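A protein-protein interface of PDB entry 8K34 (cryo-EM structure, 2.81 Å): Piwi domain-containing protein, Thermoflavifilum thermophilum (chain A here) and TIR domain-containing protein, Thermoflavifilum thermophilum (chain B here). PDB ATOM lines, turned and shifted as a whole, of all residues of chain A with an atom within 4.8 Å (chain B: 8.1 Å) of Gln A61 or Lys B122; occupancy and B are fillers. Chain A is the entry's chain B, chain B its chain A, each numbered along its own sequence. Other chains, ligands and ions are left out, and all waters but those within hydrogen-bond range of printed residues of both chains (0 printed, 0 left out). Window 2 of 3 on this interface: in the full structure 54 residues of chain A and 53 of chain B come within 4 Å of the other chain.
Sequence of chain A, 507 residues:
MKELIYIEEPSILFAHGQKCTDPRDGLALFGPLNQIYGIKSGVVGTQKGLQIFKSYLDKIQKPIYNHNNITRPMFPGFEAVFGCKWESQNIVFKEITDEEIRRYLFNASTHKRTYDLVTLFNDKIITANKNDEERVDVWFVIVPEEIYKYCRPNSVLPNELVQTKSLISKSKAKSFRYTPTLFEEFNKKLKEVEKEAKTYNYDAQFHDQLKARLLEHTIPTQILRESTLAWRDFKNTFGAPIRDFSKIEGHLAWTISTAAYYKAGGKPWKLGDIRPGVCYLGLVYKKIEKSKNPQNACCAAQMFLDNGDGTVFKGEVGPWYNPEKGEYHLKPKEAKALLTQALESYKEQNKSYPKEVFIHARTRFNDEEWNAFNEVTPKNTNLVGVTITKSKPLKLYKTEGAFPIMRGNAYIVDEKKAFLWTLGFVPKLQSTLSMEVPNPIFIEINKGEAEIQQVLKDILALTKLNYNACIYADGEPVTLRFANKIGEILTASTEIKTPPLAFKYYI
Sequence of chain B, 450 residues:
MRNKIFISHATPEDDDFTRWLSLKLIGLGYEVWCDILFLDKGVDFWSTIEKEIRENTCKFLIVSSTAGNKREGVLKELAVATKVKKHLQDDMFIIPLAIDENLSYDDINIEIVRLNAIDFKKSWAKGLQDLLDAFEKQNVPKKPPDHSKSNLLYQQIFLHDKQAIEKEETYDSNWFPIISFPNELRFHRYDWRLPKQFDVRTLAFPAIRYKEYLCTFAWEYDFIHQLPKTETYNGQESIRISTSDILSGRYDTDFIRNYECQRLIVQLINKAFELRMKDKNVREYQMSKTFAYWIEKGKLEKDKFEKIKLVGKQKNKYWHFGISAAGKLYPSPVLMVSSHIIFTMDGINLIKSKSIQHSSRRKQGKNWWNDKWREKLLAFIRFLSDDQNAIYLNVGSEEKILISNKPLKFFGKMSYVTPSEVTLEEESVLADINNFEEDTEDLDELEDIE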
ATOM      1  N   LEU A  57      27.617 -26.391  22.842  1.00  0.00           N
ATOM      2  CA  LEU A  57      27.053 -26.655  21.513  1.00  0.00           C
ATOM      3  C   LEU A  57      25.686 -26.004  21.319  1.00  0.00           C
ATOM      4  O   LEU A  57      25.387 -25.506  20.227  1.00  0.00           O
ATOM      5  CB  LEU A  57      27.002 -28.148  21.184  1.00  0.00           C
ATOM      6  CG  LEU A  57      28.311 -28.872  20.867  1.00  0.00           C
ATOM      7  CD1 LEU A  57      28.911 -28.100  19.716  1.00  0.00           C
ATOM      8  CD2 LEU A  57      29.287 -28.906  21.972  1.00  0.00           C
ATOM      9  N   ASP A  58      24.835 -25.995  22.348  1.00  0.00           N
ATOM     10  CA  ASP A  58      23.585 -25.252  22.196  1.00  0.00           C
ATOM     11  C   ASP A  58      23.864 -23.785  21.892  1.00  0.00           C
ATOM     12  O   ASP A  58      23.165 -23.165  21.082  1.00  0.00           O
ATOM     13  CB  ASP A  58      22.692 -25.388  23.430  1.00  0.00           C
ATOM     14  CG  ASP A  58      22.685 -26.788  24.000  1.00  0.00           C
ATOM     15  OD1 ASP A  58      22.822 -26.931  25.232  1.00  0.00           O
ATOM     16  OD2 ASP A  58      22.551 -27.749  23.214  1.00  0.00           O
ATOM     17  N   LYS A  59      24.891 -23.218  22.525  1.00  0.00           N
ATOM     18  CA  LYS A  59      25.283 -21.845  22.226  1.00  0.00           C
ATOM     19  C   LYS A  59      25.829 -21.714  20.807  1.00  0.00           C
ATOM     20  O   LYS A  59      25.530 -20.740  20.108  1.00  0.00           O
ATOM     21  CB  LYS A  59      26.307 -21.372  23.255  1.00  0.00           C
ATOM     22  CG  LYS A  59      25.699 -21.157  24.631  1.00  0.00           C
ATOM     23  CD  LYS A  59      26.748 -21.051  25.722  1.00  0.00           C
ATOM     24  CE  LYS A  59      27.907 -20.166  25.309  1.00  0.00           C
ATOM     25  NZ  LYS A  59      28.862 -19.979  26.435  1.00  0.00           N
ATOM     26  N   ILE A  60      26.633 -22.685  20.368  1.00  0.00           N
ATOM     27  CA  ILE A  60      27.239 -22.641  19.040  1.00  0.00           C
ATOM     28  C   ILE A  60      26.196 -22.718  17.935  1.00  0.00           C
ATOM     29  O   ILE A  60      26.355 -22.067  16.894  1.00  0.00           O
ATOM     30  CB  ILE A  60      28.276 -23.772  18.889  1.00  0.00           C
ATOM     31  CG1 ILE A  60      29.618 -23.362  19.492  1.00  0.00           C
ATOM     32  CG2 ILE A  60      28.470 -24.165  17.430  1.00  0.00           C
ATOM     33  CD1 ILE A  60      30.690 -24.403  19.295  1.00  0.00           C
ATOM     34  N   GLN A  61      25.133 -23.502  18.130  1.00  0.00           N
ATOM     35  CA  GLN A  61      24.095 -23.611  17.109  1.00  0.00           C
ATOM     36  C   GLN A  61      23.530 -22.241  16.755  1.00  0.00           C
ATOM     37  O   GLN A  61      23.390 -21.907  15.572  1.00  0.00           O
ATOM     38  CB  GLN A  61      22.980 -24.538  17.591  1.00  0.00           C
ATOM     39  CG  GLN A  61      23.426 -25.962  17.861  1.00  0.00           C
ATOM     40  CD  GLN A  61      24.268 -26.525  16.740  1.00  0.00           C
ATOM     41  OE1 GLN A  61      23.851 -26.527  15.585  1.00  0.00           O
ATOM     42  NE2 GLN A  61      25.465 -26.993  17.072  1.00  0.00           N
ATOM     43  N   LYS A  62      23.216 -21.438  17.761  1.00  0.00           N
ATOM     44  CA  LYS A  62      22.747 -20.076  17.570  1.00  0.00           C
ATOM     45  C   LYS A  62      23.928 -19.162  17.252  1.00  0.00           C
ATOM     46  O   LYS A  62      25.030 -19.376  17.761  1.00  0.00           O
ATOM     47  CB  LYS A  62      22.036 -19.589  18.826  1.00  0.00           C
ATOM     48  CG  LYS A  62      21.038 -20.588  19.384  1.00  0.00           C
ATOM     49  CD  LYS A  62      20.395 -20.076  20.659  1.00  0.00           C
ATOM     50  CE  LYS A  62      19.368 -21.061  21.189  1.00  0.00           C
ATOM     51  NZ  LYS A  62      18.734 -20.579  22.447  1.00  0.00           N
ATOM     52  N   PRO A  63      23.734 -18.144  16.417  1.00  0.00           N
ATOM     53  CA  PRO A  63      24.838 -17.228  16.113  1.00  0.00           C
ATOM     54  C   PRO A  63      25.302 -16.485  17.357  1.00  0.00           C
ATOM     55  O   PRO A  63      24.504 -16.135  18.230  1.00  0.00           O
ATOM     56  CB  PRO A  63      24.234 -16.272  15.079  1.00  0.00           C
ATOM     57  CG  PRO A  63      22.767 -16.365  15.294  1.00  0.00           C
ATOM     58  CD  PRO A  63      22.508 -17.785  15.686  1.00  0.00           C
ATOM     59  N   GLY A  77      26.979 -19.216  12.998  1.00  0.00           N
ATOM     60  CA  GLY A  77      26.495 -20.487  13.505  1.00  0.00           C
ATOM     61  C   GLY A  77      27.172 -21.585  12.705  1.00  0.00           C
ATOM     62  O   GLY A  77      27.413 -21.437  11.501  1.00  0.00           O
ATOM     63  N   PHE A  78      27.472 -22.699  13.377  1.00  0.00           N
ATOM     64  CA  PHE A  78      28.330 -23.719  12.781  1.00  0.00           C
ATOM     65  C   PHE A  78      27.789 -24.193  11.437  1.00  0.00           C
ATOM     66  O   PHE A  78      28.516 -24.224  10.439  1.00  0.00           O
ATOM     67  CB  PHE A  78      28.493 -24.894  13.744  1.00  0.00           C
ATOM     68  CG  PHE A  78      29.692 -25.752  13.457  1.00  0.00           C
ATOM     69  CD1 PHE A  78      29.752 -26.528  12.311  1.00  0.00           C
ATOM     70  CD2 PHE A  78      30.769 -25.769  14.323  1.00  0.00           C
ATOM     71  CE1 PHE A  78      30.852 -27.309  12.043  1.00  0.00           C
ATOM     72  CE2 PHE A  78      31.874 -26.547  14.054  1.00  0.00           C
ATOM     73  CZ  PHE A  78      31.914 -27.318  12.915  1.00  0.00           C
ATOM     74  N   GLU A  79      26.511 -24.567  11.392  1.00  0.00           N
ATOM     75  CA  GLU A  79      25.945 -25.065  10.145  1.00  0.00           C
ATOM     76  C   GLU A  79      25.852 -23.969   9.095  1.00  0.00           C
ATOM     77  O   GLU A  79      25.899 -24.256   7.894  1.00  0.00           O
ATOM     78  CB  GLU A  79      24.568 -25.680  10.399  1.00  0.00           C
ATOM     79  CG  GLU A  79      24.588 -26.910  11.286  1.00  0.00           C
ATOM     80  CD  GLU A  79      24.847 -26.580  12.739  1.00  0.00           C
ATOM     81  OE1 GLU A  79      24.594 -25.424  13.138  1.00  0.00           O
ATOM     82  OE2 GLU A  79      25.320 -27.469  13.476  1.00  0.00           O
ATOM     83  N   LYS A  85      26.726 -30.345  10.282  1.00  0.00           N
ATOM     84  CA  LYS A  85      26.115 -30.226  11.596  1.00  0.00           C
ATOM     85  C   LYS A  85      27.025 -30.806  12.669  1.00  0.00           C
ATOM     86  O   LYS A  85      27.750 -31.775  12.431  1.00  0.00           O
ATOM     87  CB  LYS A  85      24.758 -30.931  11.620  1.00  0.00           C
ATOM     88  CG  LYS A  85      23.773 -30.333  12.611  1.00  0.00           C
ATOM     89  CD  LYS A  85      22.337 -30.646  12.219  1.00  0.00           C
ATOM     90  CE  LYS A  85      21.370 -30.311  13.343  1.00  0.00           C
ATOM     91  NZ  LYS A  85      22.053 -29.635  14.479  1.00  0.00           N
ATOM     92  N   TRP A  86      26.987 -30.194  13.852  1.00  0.00           N
ATOM     93  CA  TRP A  86      27.706 -30.669  15.034  1.00  0.00           C
ATOM     94  C   TRP A  86      26.677 -30.712  16.158  1.00  0.00           C
ATOM     95  O   TRP A  86      26.560 -29.767  16.942  1.00  0.00           O
ATOM     96  CB  TRP A  86      28.892 -29.763  15.362  1.00  0.00           C
ATOM     97  CG  TRP A  86      29.655 -30.140  16.606  1.00  0.00           C
ATOM     98  CD1 TRP A  86      29.466 -31.242  17.387  1.00  0.00           C
ATOM     99  CD2 TRP A  86      30.743 -29.418  17.193  1.00  0.00           C
ATOM    100  NE1 TRP A  86      30.357 -31.244  18.431  1.00  0.00           N
ATOM    101  CE2 TRP A  86      31.156 -30.136  18.332  1.00  0.00           C
ATOM    102  CE3 TRP A  86      31.403 -28.230  16.872  1.00  0.00           C
ATOM    103  CZ2 TRP A  86      32.194 -29.703  19.149  1.00  0.00           C
ATOM    104  CZ3 TRP A  86      32.436 -27.804  17.682  1.00  0.00           C
ATOM    105  CH2 TRP A  86      32.822 -28.538  18.807  1.00  0.00           C
ATOM    106  N   ALA B  98      12.300 -14.358  10.678  1.00  0.00           N
ATOM    107  CA  ALA B  98      12.437 -14.065  12.103  1.00  0.00           C
ATOM    108  C   ALA B  98      13.776 -14.593  12.596  1.00  0.00           C
ATOM    109  O   ALA B  98      13.971 -15.803  12.725  1.00  0.00           O
ATOM    110  CB  ALA B  98      11.282 -14.679  12.885  1.00  0.00           C
ATOM    111  N   ILE B  99      14.707 -13.686  12.882  1.00  0.00           N
ATOM    112  CA  ILE B  99      16.033 -14.072  13.355  1.00  0.00           C
ATOM    113  C   ILE B  99      16.231 -13.810  14.837  1.00  0.00           C
ATOM    114  O   ILE B  99      17.259 -14.233  15.389  1.00  0.00           O
ATOM    115  CB  ILE B  99      17.150 -13.366  12.559  1.00  0.00           C
ATOM    116  CG1 ILE B  99      17.213 -11.887  12.931  1.00  0.00           C
ATOM    117  CG2 ILE B  99      16.901 -13.502  11.070  1.00  0.00           C
ATOM    118  CD1 ILE B  99      18.169 -11.091  12.079  1.00  0.00           C
ATOM    119  N   ASP B 100      15.300 -13.130  15.500  1.00  0.00           N
ATOM    120  CA  ASP B 100      15.484 -12.702  16.879  1.00  0.00           C
ATOM    121  C   ASP B 100      14.741 -13.643  17.818  1.00  0.00           C
ATOM    122  O   ASP B 100      13.553 -13.917  17.623  1.00  0.00           O
ATOM    123  CB  ASP B 100      14.998 -11.264  17.071  1.00  0.00           C
ATOM    124  CG  ASP B 100      15.396 -10.683  18.418  1.00  0.00           C
ATOM    125  OD1 ASP B 100      15.799 -11.450  19.318  1.00  0.00           O
ATOM    126  OD2 ASP B 100      15.318  -9.449  18.575  1.00  0.00           O
ATOM    127  N   GLU B 101      15.450 -14.133  18.835  1.00  0.00           N
ATOM    128  CA  GLU B 101      14.838 -15.011  19.824  1.00  0.00           C
ATOM    129  C   GLU B 101      13.972 -14.232  20.807  1.00  0.00           C
ATOM    130  O   GLU B 101      12.905 -14.708  21.211  1.00  0.00           O
ATOM    131  CB  GLU B 101      15.924 -15.793  20.566  1.00  0.00           C
ATOM    132  CG  GLU B 101      15.610 -16.092  22.023  1.00  0.00           C
ATOM    133  CD  GLU B 101      16.838 -16.501  22.812  1.00  0.00           C
ATOM    134  OE1 GLU B 101      17.942 -16.011  22.492  1.00  0.00           O
ATOM    135  OE2 GLU B 101      16.700 -17.310  23.753  1.00  0.00           O
ATOM    136  N   ASP B 119      11.687 -19.059  10.022  1.00  0.00           N
ATOM    137  CA  ASP B 119      12.391 -18.530  11.179  1.00  0.00           C
ATOM    138  C   ASP B 119      13.859 -18.921  11.125  1.00  0.00           C
ATOM    139  O   ASP B 119      14.207 -20.013  10.665  1.00  0.00           O
ATOM    140  CB  ASP B 119      11.764 -19.028  12.485  1.00  0.00           C
ATOM    141  CG  ASP B 119      12.289 -20.383  12.905  1.00  0.00           C
ATOM    142  OD1 ASP B 119      12.139 -21.346  12.126  1.00  0.00           O
ATOM    143  OD2 ASP B 119      12.857 -20.483  14.012  1.00  0.00           O
ATOM    144  N   PHE B 120      14.717 -18.011  11.582  1.00  0.00           N
ATOM    145  CA  PHE B 120      16.148 -18.250  11.689  1.00  0.00           C
ATOM    146  C   PHE B 120      16.613 -18.279  13.137  1.00  0.00           C
ATOM    147  O   PHE B 120      17.817 -18.191  13.396  1.00  0.00           O
ATOM    148  CB  PHE B 120      16.927 -17.180  10.921  1.00  0.00           C
ATOM    149  CG  PHE B 120      16.709 -17.203   9.435  1.00  0.00           C
ATOM    150  CD1 PHE B 120      15.487 -16.854   8.889  1.00  0.00           C
ATOM    151  CD2 PHE B 120      17.736 -17.553   8.581  1.00  0.00           C
ATOM    152  CE1 PHE B 120      15.294 -16.866   7.525  1.00  0.00           C
ATOM    153  CE2 PHE B 120      17.549 -17.560   7.217  1.00  0.00           C
ATOM    154  CZ  PHE B 120      16.326 -17.219   6.689  1.00  0.00           C
ATOM    155  N   LYS B 121      15.682 -18.389  14.087  1.00  0.00           N
ATOM    156  CA  LYS B 121      16.035 -18.294  15.500  1.00  0.00           C
ATOM    157  C   LYS B 121      16.963 -19.425  15.922  1.00  0.00           C
ATOM    158  O   LYS B 121      17.935 -19.200  16.653  1.00  0.00           O
ATOM    159  CB  LYS B 121      14.764 -18.293  16.347  1.00  0.00           C
ATOM    160  CG  LYS B 121      14.984 -18.555  17.824  1.00  0.00           C
ATOM    161  CD  LYS B 121      13.674 -18.915  18.504  1.00  0.00           C
ATOM    162  CE  LYS B 121      13.714 -18.613  19.991  1.00  0.00           C
ATOM    163  NZ  LYS B 121      12.432 -18.027  20.470  1.00  0.00           N
ATOM    164  N   LYS B 122      16.679 -20.650  15.477  1.00  0.00           N
ATOM    165  CA  LYS B 122      17.504 -21.786  15.874  1.00  0.00           C
ATOM    166  C   LYS B 122      18.861 -21.759  15.181  1.00  0.00           C
ATOM    167  O   LYS B 122      19.896 -21.962  15.826  1.00  0.00           O
ATOM    168  CB  LYS B 122      16.772 -23.092  15.572  1.00  0.00           C
ATOM    169  CG  LYS B 122      15.779 -23.503  16.644  1.00  0.00           C
ATOM    170  CD  LYS B 122      16.418 -23.483  18.022  1.00  0.00           C
ATOM    171  CE  LYS B 122      15.749 -24.480  18.953  1.00  0.00           C
ATOM    172  NZ  LYS B 122      16.536 -25.738  19.073  1.00  0.00           N
ATOM    173  N   SER B 123      18.878 -21.502  13.873  1.00  0.00           N
ATOM    174  CA  SER B 123      20.118 -21.480  13.109  1.00  0.00           C
ATOM    175  C   SER B 123      19.889 -20.865  11.736  1.00  0.00           C
ATOM    176  O   SER B 123      18.876 -21.145  11.089  1.00  0.00           O
ATOM    177  CB  SER B 123      20.687 -22.890  12.959  1.00  0.00           C
ATOM    178  OG  SER B 123      20.166 -23.521  11.804  1.00  0.00           O
ATOM    179  N   TRP B 124      20.829 -20.037  11.277  1.00  0.00           N
ATOM    180  CA  TRP B 124      20.671 -19.401   9.974  1.00  0.00           C
ATOM    181  C   TRP B 124      20.735 -20.412   8.839  1.00  0.00           C
ATOM    182  O   TRP B 124      20.198 -20.155   7.758  1.00  0.00           O
ATOM    183  CB  TRP B 124      21.733 -18.323   9.764  1.00  0.00           C
ATOM    184  CG  TRP B 124      21.696 -17.202  10.752  1.00  0.00           C
ATOM    185  CD1 TRP B 124      20.909 -17.103  11.860  1.00  0.00           C
ATOM    186  CD2 TRP B 124      22.496 -16.018  10.722  1.00  0.00           C
ATOM    187  NE1 TRP B 124      21.166 -15.929  12.519  1.00  0.00           N
ATOM    188  CE2 TRP B 124      22.140 -15.245  11.841  1.00  0.00           C
ATOM    189  CE3 TRP B 124      23.480 -15.536   9.855  1.00  0.00           C
ATOM    190  CZ2 TRP B 124      22.731 -14.018  12.116  1.00  0.00           C
ATOM    191  CZ3 TRP B 124      24.065 -14.320  10.129  1.00  0.00           C
ATOM    192  CH2 TRP B 124      23.691 -13.575  11.250  1.00  0.00           C
ATOM    193  N   ALA B 125      21.391 -21.552   9.050  1.00  0.00           N
ATOM    194  CA  ALA B 125      21.427 -22.576   8.011  1.00  0.00           C
ATOM    195  C   ALA B 125      20.054 -23.203   7.816  1.00  0.00           C
ATOM    196  O   ALA B 125      19.593 -23.376   6.681  1.00  0.00           O
ATOM    197  CB  ALA B 125      22.462 -23.644   8.359  1.00  0.00           C
ATOM    198  N   LYS B 126      19.386 -23.553   8.918  1.00  0.00           N
ATOM    199  CA  LYS B 126      18.036 -24.097   8.821  1.00  0.00           C
ATOM    200  C   LYS B 126      17.084 -23.080   8.209  1.00  0.00           C
ATOM    201  O   LYS B 126      16.253 -23.425   7.362  1.00  0.00           O
ATOM    202  CB  LYS B 126      17.547 -24.528  10.202  1.00  0.00           C
ATOM    203  CG  LYS B 126      16.688 -25.778  10.199  1.00  0.00           C
ATOM    204  CD  LYS B 126      16.254 -26.144  11.608  1.00  0.00           C
ATOM    205  CE  LYS B 126      17.435 -26.128  12.567  1.00  0.00           C
ATOM    206  NZ  LYS B 126      18.416 -27.205  12.262  1.00  0.00           N
ATOM    207  N   GLY B 127      17.197 -21.820   8.626  1.00  0.00           N
ATOM    208  CA  GLY B 127      16.361 -20.786   8.046  1.00  0.00           C
ATOM    209  C   GLY B 127      16.616 -20.597   6.564  1.00  0.00           C
ATOM    210  O   GLY B 127      15.680 -20.414   5.785  1.00  0.00           O
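The side-chain amide nitrogen (NE2) of Gln A61 is in hydrogen-bond range of the backbone carbonyl oxygen (O) of Trp A86, at 3.0 Å. OE1 of Gln A61 lies close to OE2 of Glu A79 (2.7 Å). The side-chain carboxylate (OE2) of Glu A79 lies within hydrogen-bond range of the backbone NH (N) of Trp A86. The side-chain hydroxyl (OG) of Ser B123 sits at hydrogen-bond distance from the backbone NH (N) of Lys B126. The backbone carbonyl oxygen (O) of Leu A57 sits close to the side-chain amide nitrogen (NE2) of Gln A61 (3.5 Å).
Among the printed residues, pairs that only touch across the chains: Gln A61 with Lys B122 (3.5 Å), Gln A61 with Ser B123 (3.9 Å), Lys A62 with Lys B122 (3.8 Å), Pro A63 with Trp B124 (3.2 Å) and Glu A79 with Ala B125 (3.5 Å).
Gln A61 touches two residues of chain B. Lys B122 touches two residues of chain A. Of the printed residues of chain B, Glu A79 touches Ala B125 (3.5 Å). Printed residues of chain A within 4 Å of Trp B124: Pro A63. Of the printed residues of chain A, Ser B123 touches Gln A61 (3.9 Å). Of the printed residues of chain B, Pro A63 touches Trp B124. Printed residues of chain A within 4 Å of Ala B125: Glu A79 (3.5 Å). The nearest printed residue of chain A that does not touch Lys B122 is Pro A63 (4.9 Å). The nearest printed residue of chain A that does not touch Ala B125 is Phe A78 (6.2 Å).
Hydrophobic or aromatic side chains of chain B that line the printed part of chain A: Trp B124 and Ala B125. Hydrophobic or aromatic side chains of chain A that line the printed part of chain B: Pro A63. Among the printed residues, 5 pairs touch across the chains. Among the printed residues, no Asp or Glu carboxylate lies within 4 Å of a Lys or Arg side-chain nitrogen of the other chain.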
